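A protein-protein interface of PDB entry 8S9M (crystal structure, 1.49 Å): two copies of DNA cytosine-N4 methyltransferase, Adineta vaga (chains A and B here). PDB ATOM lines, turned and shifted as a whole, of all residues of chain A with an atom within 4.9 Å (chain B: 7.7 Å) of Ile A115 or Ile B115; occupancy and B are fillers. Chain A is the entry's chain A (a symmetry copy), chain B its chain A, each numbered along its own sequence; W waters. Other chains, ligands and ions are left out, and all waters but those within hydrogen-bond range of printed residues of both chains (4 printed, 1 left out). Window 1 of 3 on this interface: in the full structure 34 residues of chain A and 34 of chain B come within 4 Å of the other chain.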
ATOM      1  N   THR A 113       6.905  16.483  20.486  1.00  0.00           N
ATOM      2  CA  THR A 113       8.235  16.553  21.076  1.00  0.00           C
ATOM      3  C   THR A 113       9.163  15.622  20.311  1.00  0.00           C
ATOM      4  O   THR A 113       8.887  14.422  20.183  1.00  0.00           O
ATOM      5  CB  THR A 113       8.238  16.196  22.560  1.00  0.00           C
ATOM      6  OG1 THR A 113       7.378  17.093  23.269  1.00  0.00           O
ATOM      7  CG2 THR A 113       9.660  16.332  23.104  1.00  0.00           C
ATOM      8  N   ILE A 114      10.253  16.171  19.815  1.00  0.00           N
ATOM      9  CA  ILE A 114      11.276  15.418  19.103  1.00  0.00           C
ATOM     10  C   ILE A 114      12.436  15.149  20.049  1.00  0.00           C
ATOM     11  O   ILE A 114      12.786  15.993  20.878  1.00  0.00           O
ATOM     12  CB  ILE A 114      11.736  16.214  17.867  1.00  0.00           C
ATOM     13  CG1 ILE A 114      10.596  16.324  16.839  1.00  0.00           C
ATOM     14  CG2 ILE A 114      13.003  15.609  17.256  1.00  0.00           C
ATOM     15  CD1 ILE A 114      10.628  17.617  16.059  1.00  0.00           C
ATOM     16  N   ILE A 115      13.038  13.973  19.928  1.00  0.00           N
ATOM     17  CA  ILE A 115      14.155  13.571  20.771  1.00  0.00           C
ATOM     18  C   ILE A 115      15.439  13.738  19.971  1.00  0.00           C
ATOM     19  O   ILE A 115      15.615  13.097  18.930  1.00  0.00           O
ATOM     20  CB  ILE A 115      13.977  12.119  21.243  1.00  0.00           C
ATOM     21  CG1 ILE A 115      12.691  11.982  22.073  1.00  0.00           C
ATOM     22  CG2 ILE A 115      15.210  11.628  21.999  1.00  0.00           C
ATOM     23  CD1 ILE A 115      12.647  12.864  23.310  1.00  0.00           C
ATOM     24  N   TRP A 116      16.340  14.592  20.453  1.00  0.00           N
ATOM     25  CA  TRP A 116      17.681  14.719  19.884  1.00  0.00           C
ATOM     26  C   TRP A 116      18.614  13.798  20.667  1.00  0.00           C
ATOM     27  O   TRP A 116      18.952  14.071  21.828  1.00  0.00           O
ATOM     28  CB  TRP A 116      18.148  16.177  19.922  1.00  0.00           C
ATOM     29  CG  TRP A 116      19.563  16.390  19.456  1.00  0.00           C
ATOM     30  CD1 TRP A 116      20.343  15.529  18.720  1.00  0.00           C
ATOM     31  CD2 TRP A 116      20.375  17.545  19.709  1.00  0.00           C
ATOM     32  NE1 TRP A 116      21.589  16.076  18.525  1.00  0.00           N
ATOM     33  CE2 TRP A 116      21.632  17.313  19.115  1.00  0.00           C
ATOM     34  CE3 TRP A 116      20.166  18.742  20.402  1.00  0.00           C
ATOM     35  CZ2 TRP A 116      22.671  18.239  19.180  1.00  0.00           C
ATOM     36  CZ3 TRP A 116      21.195  19.669  20.455  1.00  0.00           C
ATOM     37  CH2 TRP A 116      22.435  19.411  19.852  1.00  0.00           C
ATOM     38  N   ASP A 117      19.005  12.691  20.035  1.00  0.00           N
ATOM     39  CA  ASP A 117      19.946  11.732  20.614  1.00  0.00           C
ATOM     40  C   ASP A 117      21.358  12.194  20.256  1.00  0.00           C
ATOM     41  O   ASP A 117      21.790  12.070  19.103  1.00  0.00           O
ATOM     42  CB  ASP A 117      19.646  10.341  20.053  1.00  0.00           C
ATOM     43  CG  ASP A 117      20.619   9.279  20.527  1.00  0.00           C
ATOM     44  OD1 ASP A 117      21.513   9.583  21.349  1.00  0.00           O
ATOM     45  OD2 ASP A 117      20.488   8.122  20.062  1.00  0.00           O
ATOM     46  N   VAL A 133      20.264  13.011  25.928  1.00  0.00           N
ATOM     47  CA  VAL A 133      19.116  13.427  25.125  1.00  0.00           C
ATOM     48  C   VAL A 133      18.780  14.885  25.407  1.00  0.00           C
ATOM     49  O   VAL A 133      18.747  15.320  26.566  1.00  0.00           O
ATOM     50  CB  VAL A 133      17.896  12.525  25.399  1.00  0.00           C
ATOM     51  CG1 VAL A 133      16.597  13.239  25.033  1.00  0.00           C
ATOM     52  CG2 VAL A 133      18.037  11.225  24.634  1.00  0.00           C
ATOM     53  N   GLU A 134      18.517  15.638  24.340  1.00  0.00           N
ATOM     54  CA  GLU A 134      17.842  16.918  24.445  1.00  0.00           C
ATOM     55  C   GLU A 134      16.505  16.819  23.727  1.00  0.00           C
ATOM     56  O   GLU A 134      16.270  15.908  22.929  1.00  0.00           O
ATOM     57  CB  GLU A 134      18.688  18.064  23.881  1.00  0.00           C
ATOM     58  CG  GLU A 134      19.982  18.242  24.636  1.00  0.00           C
ATOM     59  CD  GLU A 134      20.662  19.557  24.349  1.00  0.00           C
ATOM     60  OE1 GLU A 134      20.002  20.478  23.817  1.00  0.00           O
ATOM     61  OE2 GLU A 134      21.867  19.662  24.653  1.00  0.00           O
ATOM     62  N   LYS A 135      15.603  17.722  24.060  1.00  0.00           N
ATOM     63  CA  LYS A 135      14.289  17.729  23.448  1.00  0.00           C
ATOM     64  C   LYS A 135      14.183  18.893  22.479  1.00  0.00           C
ATOM     65  O   LYS A 135      14.758  19.964  22.703  1.00  0.00           O
ATOM     66  CB  LYS A 135      13.183  17.792  24.502  1.00  0.00           C
ATOM     67  CG  LYS A 135      13.125  16.512  25.312  1.00  0.00           C
ATOM     68  CD  LYS A 135      11.950  16.470  26.246  1.00  0.00           C
ATOM     69  CE  LYS A 135      12.272  17.156  27.553  1.00  0.00           C
ATOM     70  NZ  LYS A 135      11.415  16.613  28.660  1.00  0.00           N
ATOM     71  N   VAL A 164      10.824  10.284  15.208  1.00  0.00           N
ATOM     72  CA  VAL A 164      10.828  11.220  16.328  1.00  0.00           C
ATOM     73  C   VAL A 164      12.149  11.261  17.087  1.00  0.00           C
ATOM     74  O   VAL A 164      12.345  12.165  17.911  1.00  0.00           O
ATOM     75  CB  VAL A 164       9.597  10.912  17.200  1.00  0.00           C
ATOM     76  CG1 VAL A 164       9.794   9.608  17.956  1.00  0.00           C
ATOM     77  CG2 VAL A 164       9.284  12.053  18.129  1.00  0.00           C
ATOM     78  N   ILE A 165      13.068  10.321  16.846  1.00  0.00           N
ATOM     79  CA  ILE A 165      14.429  10.410  17.367  1.00  0.00           C
ATOM     80  C   ILE A 165      15.354  10.794  16.227  1.00  0.00           C
ATOM     81  O   ILE A 165      15.381  10.115  15.192  1.00  0.00           O
ATOM     82  CB  ILE A 165      14.902   9.097  18.014  1.00  0.00           C
ATOM     83  CG1 ILE A 165      13.984   8.686  19.164  1.00  0.00           C
ATOM     84  CG2 ILE A 165      16.323   9.269  18.559  1.00  0.00           C
ATOM     85  CD1 ILE A 165      14.398   7.343  19.804  1.00  0.00           C
ATOM     86  N   TRP A 166      16.115  11.871  16.421  1.00  0.00           N
ATOM     87  CA  TRP A 166      17.148  12.292  15.481  1.00  0.00           C
ATOM     88  C   TRP A 166      18.511  12.001  16.095  1.00  0.00           C
ATOM     89  O   TRP A 166      18.869  12.583  17.129  1.00  0.00           O
ATOM     90  CB  TRP A 166      17.045  13.784  15.175  1.00  0.00           C
ATOM     91  CG  TRP A 166      15.763  14.230  14.586  1.00  0.00           C
ATOM     92  CD1 TRP A 166      14.742  13.447  14.110  1.00  0.00           C
ATOM     93  CD2 TRP A 166      15.338  15.580  14.440  1.00  0.00           C
ATOM     94  NE1 TRP A 166      13.712  14.243  13.653  1.00  0.00           N
ATOM     95  CE2 TRP A 166      14.053  15.557  13.855  1.00  0.00           C
ATOM     96  CE3 TRP A 166      15.922  16.817  14.744  1.00  0.00           C
ATOM     97  CZ2 TRP A 166      13.342  16.721  13.575  1.00  0.00           C
ATOM     98  CZ3 TRP A 166      15.216  17.969  14.463  1.00  0.00           C
ATOM     99  CH2 TRP A 166      13.940  17.914  13.885  1.00  0.00           C
ATOM    100  N   ASP B  89       3.051   9.806  24.565  1.00  0.00           N
ATOM    101  CA  ASP B  89       2.348  10.969  24.038  1.00  0.00           C
ATOM    102  C   ASP B  89       1.215  10.510  23.128  1.00  0.00           C
ATOM    103  O   ASP B  89       1.405   9.659  22.251  1.00  0.00           O
ATOM    104  CB  ASP B  89       3.329  11.843  23.253  1.00  0.00           C
ATOM    105  CG  ASP B  89       4.325  12.562  24.149  1.00  0.00           C
ATOM    106  OD1 ASP B  89       4.157  12.520  25.387  1.00  0.00           O
ATOM    107  OD2 ASP B  89       5.280  13.171  23.611  1.00  0.00           O
ATOM    108  N   GLU B 100       2.669  14.073  30.828  1.00  0.00           N
ATOM    109  CA  GLU B 100       3.100  15.067  31.802  1.00  0.00           C
ATOM    110  C   GLU B 100       1.982  16.021  32.195  1.00  0.00           C
ATOM    111  O   GLU B 100       2.042  16.615  33.275  1.00  0.00           O
ATOM    112  CB  GLU B 100       4.298  15.860  31.266  1.00  0.00           C
ATOM    113  CG  GLU B 100       5.616  15.086  31.202  1.00  0.00           C
ATOM    114  CD  GLU B 100       5.840  14.360  29.876  1.00  0.00           C
ATOM    115  OE1 GLU B 100       4.855  14.049  29.173  1.00  0.00           O
ATOM    116  OE2 GLU B 100       7.016  14.101  29.536  1.00  0.00           O
ATOM    117  N   GLN B 112      13.699  10.756  36.656  1.00  0.00           N
ATOM    118  CA  GLN B 112      14.240  10.845  35.306  1.00  0.00           C
ATOM    119  C   GLN B 112      13.197  10.301  34.341  1.00  0.00           C
ATOM    120  O   GLN B 112      12.423   9.407  34.692  1.00  0.00           O
ATOM    121  CB  GLN B 112      15.541  10.037  35.175  1.00  0.00           C
ATOM    122  CG  GLN B 112      16.295  10.261  33.868  1.00  0.00           C
ATOM    123  CD  GLN B 112      17.654   9.587  33.850  1.00  0.00           C
ATOM    124  OE1 GLN B 112      17.841   8.529  34.449  1.00  0.00           O
ATOM    125  NE2 GLN B 112      18.610  10.196  33.151  1.00  0.00           N
ATOM    126  N   THR B 113      13.171  10.849  33.129  1.00  0.00           N
ATOM    127  CA  THR B 113      12.367  10.279  32.056  1.00  0.00           C
ATOM    128  C   THR B 113      13.272   9.471  31.137  1.00  0.00           C
ATOM    129  O   THR B 113      14.262   9.994  30.610  1.00  0.00           O
ATOM    130  CB  THR B 113      11.620  11.343  31.256  1.00  0.00           C
ATOM    131  OG1 THR B 113      10.757  12.079  32.128  1.00  0.00           O
ATOM    132  CG2 THR B 113      10.776  10.658  30.180  1.00  0.00           C
ATOM    133  N   ILE B 114      12.929   8.214  30.948  1.00  0.00           N
ATOM    134  CA  ILE B 114      13.649   7.313  30.059  1.00  0.00           C
ATOM    135  C   ILE B 114      12.887   7.205  28.747  1.00  0.00           C
ATOM    136  O   ILE B 114      11.654   7.198  28.730  1.00  0.00           O
ATOM    137  CB  ILE B 114      13.802   5.936  30.733  1.00  0.00           C
ATOM    138  CG1 ILE B 114      14.723   6.034  31.961  1.00  0.00           C
ATOM    139  CG2 ILE B 114      14.286   4.881  29.735  1.00  0.00           C
ATOM    140  CD1 ILE B 114      14.342   5.072  33.061  1.00  0.00           C
ATOM    141  N   ILE B 115      13.619   7.116  27.643  1.00  0.00           N
ATOM    142  CA  ILE B 115      13.030   7.017  26.316  1.00  0.00           C
ATOM    143  C   ILE B 115      13.102   5.563  25.870  1.00  0.00           C
ATOM    144  O   ILE B 115      14.195   5.001  25.746  1.00  0.00           O
ATOM    145  CB  ILE B 115      13.766   7.939  25.331  1.00  0.00           C
ATOM    146  CG1 ILE B 115      13.653   9.403  25.786  1.00  0.00           C
ATOM    147  CG2 ILE B 115      13.265   7.736  23.902  1.00  0.00           C
ATOM    148  CD1 ILE B 115      12.228   9.915  25.899  1.00  0.00           C
ATOM    149  N   TRP B 116      11.944   4.952  25.623  1.00  0.00           N
ATOM    150  CA  TRP B 116      11.874   3.620  25.025  1.00  0.00           C
ATOM    151  C   TRP B 116      11.734   3.789  23.514  1.00  0.00           C
ATOM    152  O   TRP B 116      10.677   4.198  23.015  1.00  0.00           O
ATOM    153  CB  TRP B 116      10.714   2.820  25.624  1.00  0.00           C
ATOM    154  CG  TRP B 116      10.496   1.472  24.992  1.00  0.00           C
ATOM    155  CD1 TRP B 116      11.372   0.761  24.206  1.00  0.00           C
ATOM    156  CD2 TRP B 116       9.307   0.674  25.084  1.00  0.00           C
ATOM    157  NE1 TRP B 116      10.787  -0.413  23.794  1.00  0.00           N
ATOM    158  CE2 TRP B 116       9.524  -0.493  24.324  1.00  0.00           C
ATOM    159  CE3 TRP B 116       8.072   0.847  25.718  1.00  0.00           C
ATOM    160  CZ2 TRP B 116       8.559  -1.489  24.191  1.00  0.00           C
ATOM    161  CZ3 TRP B 116       7.117  -0.150  25.597  1.00  0.00           C
ATOM    162  CH2 TRP B 116       7.363  -1.302  24.835  1.00  0.00           C
ATOM    163  N   ASP B 117      12.817   3.498  22.793  1.00  0.00           N
ATOM    164  CA  ASP B 117      12.838   3.544  21.331  1.00  0.00           C
ATOM    165  C   ASP B 117      12.375   2.182  20.817  1.00  0.00           C
ATOM    166  O   ASP B 117      13.116   1.193  20.892  1.00  0.00           O
ATOM    167  CB  ASP B 117      14.257   3.874  20.865  1.00  0.00           C
ATOM    168  CG  ASP B 117      14.410   3.868  19.356  1.00  0.00           C
ATOM    169  OD1 ASP B 117      13.407   3.667  18.634  1.00  0.00           O
ATOM    170  OD2 ASP B 117      15.557   4.061  18.887  1.00  0.00           O
ATOM    171  N   ARG B 118      11.145   2.129  20.312  1.00  0.00           N
ATOM    172  CA  ARG B 118      10.597   0.902  19.741  1.00  0.00           C
ATOM    173  C   ARG B 118      11.015   0.665  18.294  1.00  0.00           C
ATOM    174  O   ARG B 118      10.663  -0.378  17.729  1.00  0.00           O
ATOM    175  CB  ARG B 118       9.069   0.907  19.848  1.00  0.00           C
ATOM    176  CG  ARG B 118       8.565   0.932  21.281  1.00  0.00           C
ATOM    177  CD  ARG B 118       7.089   1.314  21.366  1.00  0.00           C
ATOM    178  NE  ARG B 118       6.229   0.509  20.503  1.00  0.00           N
ATOM    179  CZ  ARG B 118       5.424  -0.458  20.928  1.00  0.00           C
ATOM    180  NH1 ARG B 118       5.361  -0.793  22.206  1.00  0.00           N
ATOM    181  NH2 ARG B 118       4.664  -1.107  20.049  1.00  0.00           N
ATOM    182  N   TYR B 132       7.432   6.418  17.259  1.00  0.00           N
ATOM    183  CA  TYR B 132       7.822   5.104  17.766  1.00  0.00           C
ATOM    184  C   TYR B 132       8.468   5.158  19.153  1.00  0.00           C
ATOM    185  O   TYR B 132       9.124   4.192  19.558  1.00  0.00           O
ATOM    186  CB  TYR B 132       8.728   4.371  16.766  1.00  0.00           C
ATOM    187  CG  TYR B 132       9.917   5.186  16.314  1.00  0.00           C
ATOM    188  CD1 TYR B 132      10.955   5.482  17.184  1.00  0.00           C
ATOM    189  CD2 TYR B 132       9.997   5.668  15.019  1.00  0.00           C
ATOM    190  CE1 TYR B 132      12.037   6.244  16.776  1.00  0.00           C
ATOM    191  CE2 TYR B 132      11.070   6.429  14.603  1.00  0.00           C
ATOM    192  CZ  TYR B 132      12.086   6.717  15.487  1.00  0.00           C
ATOM    193  OH  TYR B 132      13.158   7.476  15.075  1.00  0.00           O
ATOM    194  N   VAL B 133       8.309   6.260  19.884  1.00  0.00           N
ATOM    195  CA  VAL B 133       8.870   6.400  21.225  1.00  0.00           C
ATOM    196  C   VAL B 133       7.764   6.311  22.269  1.00  0.00           C
ATOM    197  O   VAL B 133       6.695   6.920  22.121  1.00  0.00           O
ATOM    198  CB  VAL B 133       9.641   7.729  21.364  1.00  0.00           C
ATOM    199  CG1 VAL B 133       9.744   8.149  22.829  1.00  0.00           C
ATOM    200  CG2 VAL B 133      11.014   7.592  20.739  1.00  0.00           C
ATOM    201  N   GLU B 134       8.029   5.556  23.333  1.00  0.00           N
ATOM    202  CA  GLU B 134       7.256   5.649  24.558  1.00  0.00           C
ATOM    203  C   GLU B 134       8.168   6.152  25.667  1.00  0.00           C
ATOM    204  O   GLU B 134       9.395   6.120  25.553  1.00  0.00           O
ATOM    205  CB  GLU B 134       6.612   4.312  24.937  1.00  0.00           C
ATOM    206  CG  GLU B 134       5.633   3.835  23.892  1.00  0.00           C
ATOM    207  CD  GLU B 134       4.731   2.730  24.383  1.00  0.00           C
ATOM    208  OE1 GLU B 134       4.629   2.532  25.615  1.00  0.00           O
ATOM    209  OE2 GLU B 134       4.129   2.054  23.526  1.00  0.00           O
ATOM    210  N   LYS B 135       7.564   6.677  26.716  1.00  0.00           N
ATOM    211  CA  LYS B 135       8.325   7.194  27.836  1.00  0.00           C
ATOM    212  C   LYS B 135       8.198   6.251  29.019  1.00  0.00           C
ATOM    213  O   LYS B 135       7.151   5.628  29.229  1.00  0.00           O
ATOM    214  CB  LYS B 135       7.876   8.607  28.211  1.00  0.00           C
ATOM    215  CG  LYS B 135       8.235   9.601  27.125  1.00  0.00           C
ATOM    216  CD  LYS B 135       7.956  11.021  27.525  1.00  0.00           C
ATOM    217  CE  LYS B 135       6.520  11.394  27.242  1.00  0.00           C
ATOM    218  NZ  LYS B 135       6.386  12.876  27.044  1.00  0.00           N
ATOM    219  N   ILE B 136       9.281   6.121  29.766  1.00  0.00           N
ATOM    220  CA  ILE B 136       9.261   5.407  31.028  1.00  0.00           C
ATOM    221  C   ILE B 136       9.616   6.432  32.089  1.00  0.00           C
ATOM    222  O   ILE B 136      10.768   6.869  32.180  1.00  0.00           O
ATOM    223  CB  ILE B 136      10.234   4.219  31.045  1.00  0.00           C
ATOM    224  CG1 ILE B 136       9.902   3.256  29.891  1.00  0.00           C
ATOM    225  CG2 ILE B 136      10.168   3.530  32.401  1.00  0.00           C
ATOM    226  CD1 ILE B 136      10.964   2.217  29.626  1.00  0.00           C
ATOM    227  N   PHE B 137       8.626   6.842  32.867  1.00  0.00           N
ATOM    228  CA  PHE B 137       8.841   7.803  33.936  1.00  0.00           C
ATOM    229  C   PHE B 137       9.365   7.076  35.165  1.00  0.00           C
ATOM    230  O   PHE B 137       8.690   6.206  35.712  1.00  0.00           O
ATOM    231  CB  PHE B 137       7.535   8.521  34.241  1.00  0.00           C
ATOM    232  CG  PHE B 137       7.039   9.331  33.091  1.00  0.00           C
ATOM    233  CD1 PHE B 137       7.535  10.598  32.862  1.00  0.00           C
ATOM    234  CD2 PHE B 137       6.099   8.808  32.218  1.00  0.00           C
ATOM    235  CE1 PHE B 137       7.084  11.350  31.784  1.00  0.00           C
ATOM    236  CE2 PHE B 137       5.646   9.547  31.144  1.00  0.00           C
ATOM    237  CZ  PHE B 137       6.135  10.822  30.925  1.00  0.00           C
ATOM    238  N   GLY B 163      22.231   4.131  29.166  1.00  0.00           N
ATOM    239  CA  GLY B 163      21.829   5.450  28.734  1.00  0.00           C
ATOM    240  C   GLY B 163      20.327   5.670  28.848  1.00  0.00           C
ATOM    241  O   GLY B 163      19.541   4.767  29.128  1.00  0.00           O
ATOM    242  N   VAL B 164      19.930   6.918  28.600  1.00  0.00           N
ATOM    243  CA  VAL B 164      18.531   7.304  28.761  1.00  0.00           C
ATOM    244  C   VAL B 164      17.637   6.859  27.610  1.00  0.00           C
ATOM    245  O   VAL B 164      16.407   6.936  27.736  1.00  0.00           O
ATOM    246  CB  VAL B 164      18.494   8.815  29.054  1.00  0.00           C
ATOM    247  CG1 VAL B 164      18.837   9.608  27.803  1.00  0.00           C
ATOM    248  CG2 VAL B 164      17.168   9.230  29.631  1.00  0.00           C
ATOM    249  N   ILE B 165      18.200   6.393  26.490  1.00  0.00           N
ATOM    250  CA  ILE B 165      17.421   5.753  25.436  1.00  0.00           C
ATOM    251  C   ILE B 165      17.668   4.256  25.500  1.00  0.00           C
ATOM    252  O   ILE B 165      18.823   3.814  25.448  1.00  0.00           O
ATOM    253  CB  ILE B 165      17.768   6.288  24.036  1.00  0.00           C
ATOM    254  CG1 ILE B 165      17.531   7.794  23.946  1.00  0.00           C
ATOM    255  CG2 ILE B 165      16.898   5.592  22.984  1.00  0.00           C
ATOM    256  CD1 ILE B 165      17.918   8.376  22.570  1.00  0.00           C
ATOM    257  N   TRP B 166      16.587   3.483  25.599  1.00  0.00           N
ATOM    258  CA  TRP B 166      16.646   2.027  25.537  1.00  0.00           C
ATOM    259  C   TRP B 166      16.066   1.574  24.203  1.00  0.00           C
ATOM    260  O   TRP B 166      14.874   1.784  23.935  1.00  0.00           O
ATOM    261  CB  TRP B 166      15.846   1.390  26.671  1.00  0.00           C
ATOM    262  CG  TRP B 166      16.280   1.750  28.040  1.00  0.00           C
ATOM    263  CD1 TRP B 166      17.416   2.423  28.409  1.00  0.00           C
ATOM    264  CD2 TRP B 166      15.559   1.487  29.238  1.00  0.00           C
ATOM    265  NE1 TRP B 166      17.450   2.571  29.781  1.00  0.00           N
ATOM    266  CE2 TRP B 166      16.314   2.011  30.308  1.00  0.00           C
ATOM    267  CE3 TRP B 166      14.342   0.850  29.515  1.00  0.00           C
ATOM    268  CZ2 TRP B 166      15.889   1.926  31.632  1.00  0.00           C
ATOM    269  CZ3 TRP B 166      13.924   0.764  30.828  1.00  0.00           C
ATOM    270  CH2 TRP B 166      14.695   1.298  31.870  1.00  0.00           C
ATOM    271  N   ARG B 167      16.893   0.915  23.391  1.00  0.00           N
ATOM    272  CA  ARG B 167      16.490   0.386  22.085  1.00  0.00           C
ATOM    273  C   ARG B 167      15.999  -1.050  22.255  1.00  0.00           C
ATOM    274  O   ARG B 167      16.797  -1.987  22.242  1.00  0.00           O
ATOM    275  CB  ARG B 167      17.685   0.391  21.134  1.00  0.00           C
ATOM    276  CG  ARG B 167      17.707   1.558  20.168  1.00  0.00           C
ATOM    277  CD  ARG B 167      18.203   2.832  20.832  1.00  0.00           C
ATOM    278  NE  ARG B 167      18.012   3.962  19.935  1.00  0.00           N
ATOM    279  CZ  ARG B 167      18.704   5.091  19.972  1.00  0.00           C
ATOM    280  NH1 ARG B 167      19.648   5.302  20.877  1.00  0.00           N
ATOM    281  NH2 ARG B 167      18.432   6.046  19.093  1.00  0.00           N
ATOM    282  N   ILE B 168      14.687  -1.224  22.417  1.00  0.00           N
ATOM    283  CA  ILE B 168      14.105  -2.533  22.665  1.00  0.00           C
ATOM    284  C   ILE B 168      12.946  -2.723  21.695  1.00  0.00           C
ATOM    285  O   ILE B 168      11.976  -1.962  21.740  1.00  0.00           O
ATOM    286  CB  ILE B 168      13.619  -2.699  24.115  1.00  0.00           C
ATOM    287  CG1 ILE B 168      14.741  -2.353  25.114  1.00  0.00           C
ATOM    288  CG2 ILE B 168      13.103  -4.113  24.315  1.00  0.00           C
ATOM    289  CD1 ILE B 168      14.271  -2.212  26.572  1.00  0.00           C
HETATM  290  O   HOH W   1       5.137  14.200  21.130  1.00  0.00           O
HETATM  291  O   HOH W   2      16.384   7.562  14.888  1.00  0.00           O
HETATM  292  O   HOH W   3      22.356   6.809  21.731  1.00  0.00           O
HETATM  293  O   HOH W   4       5.239  15.837  24.236  1.00  0.00           O
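OH of Tyr B132 lies within hydrogen-bond range of N of Ile A165 (3.4 Å).
The side-chain carboxylate (OD2) of Asp A117 is in salt-bridge range of the guanidinium group (NH1) of Arg B167.
N of Ile B115 lies within hydrogen-bond range of O of Val B164 (2.8 Å).
The side-chain carboxylate (OD2) of Asp B117 is in salt-bridge range of the guanidinium group (NE) of Arg B167 (2.7 Å).
O of Asp B117 lies within hydrogen-bond range of N of Ile B168 (3.3 Å).
N of Arg B118 lies within hydrogen-bond range of O of Tyr B132 (3.0 Å).
The backbone carbonyl oxygen of Ile A115 lies within hydrogen-bond range of the backbone NH of Trp A166 (2.8 Å).
O of Trp A166 lies within hydrogen-bond range of N of Asp A117.
Among the printed residues, pairs that only touch across the chains: Ile A165 with Asp B117 (3.5 Å), Asp A117 with Ile B165 (3.5 Å), Ile A165 with Val B133 (3.5 Å), Val A133 with Ile B165 (3.5 Å), Val A133 with Val B164 (3.6 Å), Val A164 with Val B133 (3.6 Å), Val A164 with Tyr B132 (3.7 Å), Ile A165 with Arg B167 (3.9 Å) and Ile A115 with Ile B115 (3.9 Å).
Ile A115 touches just one residue of chain B: Ile B115 (3.9 Å).
Ile B115 touches just one residue of chain A: Ile A115 (3.9 Å).
Of the printed residues of chain A, Val B164 touches Val A133 (3.6 Å).
Of the printed residues of chain B, Ile A165 touches Asp B117 (3.5 Å), Tyr B132 (3.4 Å), Val B133 (3.5 Å) and Arg B167 (3.9 Å).
Of the printed residues of chain A, Val B133 touches Val A164 and Ile A165.
Printed residues of chain A within 4 Å of Arg B167: Asp A117 and Ile A165.
Of the printed residues of chain B, Val A164 touches Tyr B132 and Val B133.
Gly B163 touches none of the printed residues of chain A.
The nearest residue of chain B that does not touch Ile A115 is Ile B165 (4.3 Å).
The nearest residue of chain A that does not touch Ile B115 is Ile A165 (4.3 Å).
The nearest printed residue of chain A that does not touch Asp B117 is Asp A117 (6.5 Å).
Printed residues of chain A that touch a printed residue of chain B: Ile A115, Asp A117, Val A133, Val A164 and Ile A165.
Hydrophobic or aromatic side chains of chain A that line the printed part of chain B: Ile A115, Val A133, Val A164 and Ile A165.
Printed residues of chain B that touch a printed residue of chain A: Ile B115, Asp B117, Tyr B132, Val B133, Val B164, Ile B165 and Arg B167.
Hydrophobic or aromatic side chains of chain B that line the printed part of chain A: Ile B115, Tyr B132, Val B133, Val B164 and Ile B165.
Among the printed residues, 11 pairs touch across the chains.
Among the printed residues, Asp or Glu carboxylates within 4 Å of a Lys or Arg side-chain nitrogen of the other chain: Asp A117 with Arg B167.
Ile A115 touches its own counterpart, Ile B115.
Asp A117 touches Ile B165, and with the chains exchanged Ile A165 touches Asp B117.
Val A133 touches Val B164, and with the chains exchanged Val A164 touches Val B133.
Val A133 touches Ile B165, and with the chains exchanged Ile A165 touches Val B133.
Positions printed for both chains: 113, 114, 115, 116, 117, 133, 134, 135, 164, 165 and 166.
Of the 11 pairs that touch across the chains among the printed residues, 7 have their exchanged pair printed and touching as well.
Water W4 bridges the side-chain hydroxyl (OG1) of Thr A113 (2.7 Å) and the side-chain carboxylate (OD2) of Asp B89 (2.7 Å).
Water W1 bridges the side-chain carboxylate of Asp B89 (2.7 Å) and the backbone NH of Thr A113 (3.0 Å).
Water W2 lies within hydrogen-bond range of O of Ile A165 (2.8 Å) and OH of Tyr B132 (3.2 Å).
Water W3 bridges the side-chain carboxylate of Asp A117 (2.8 Å) and the guanidinium group of Arg B167 (3.2 Å).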
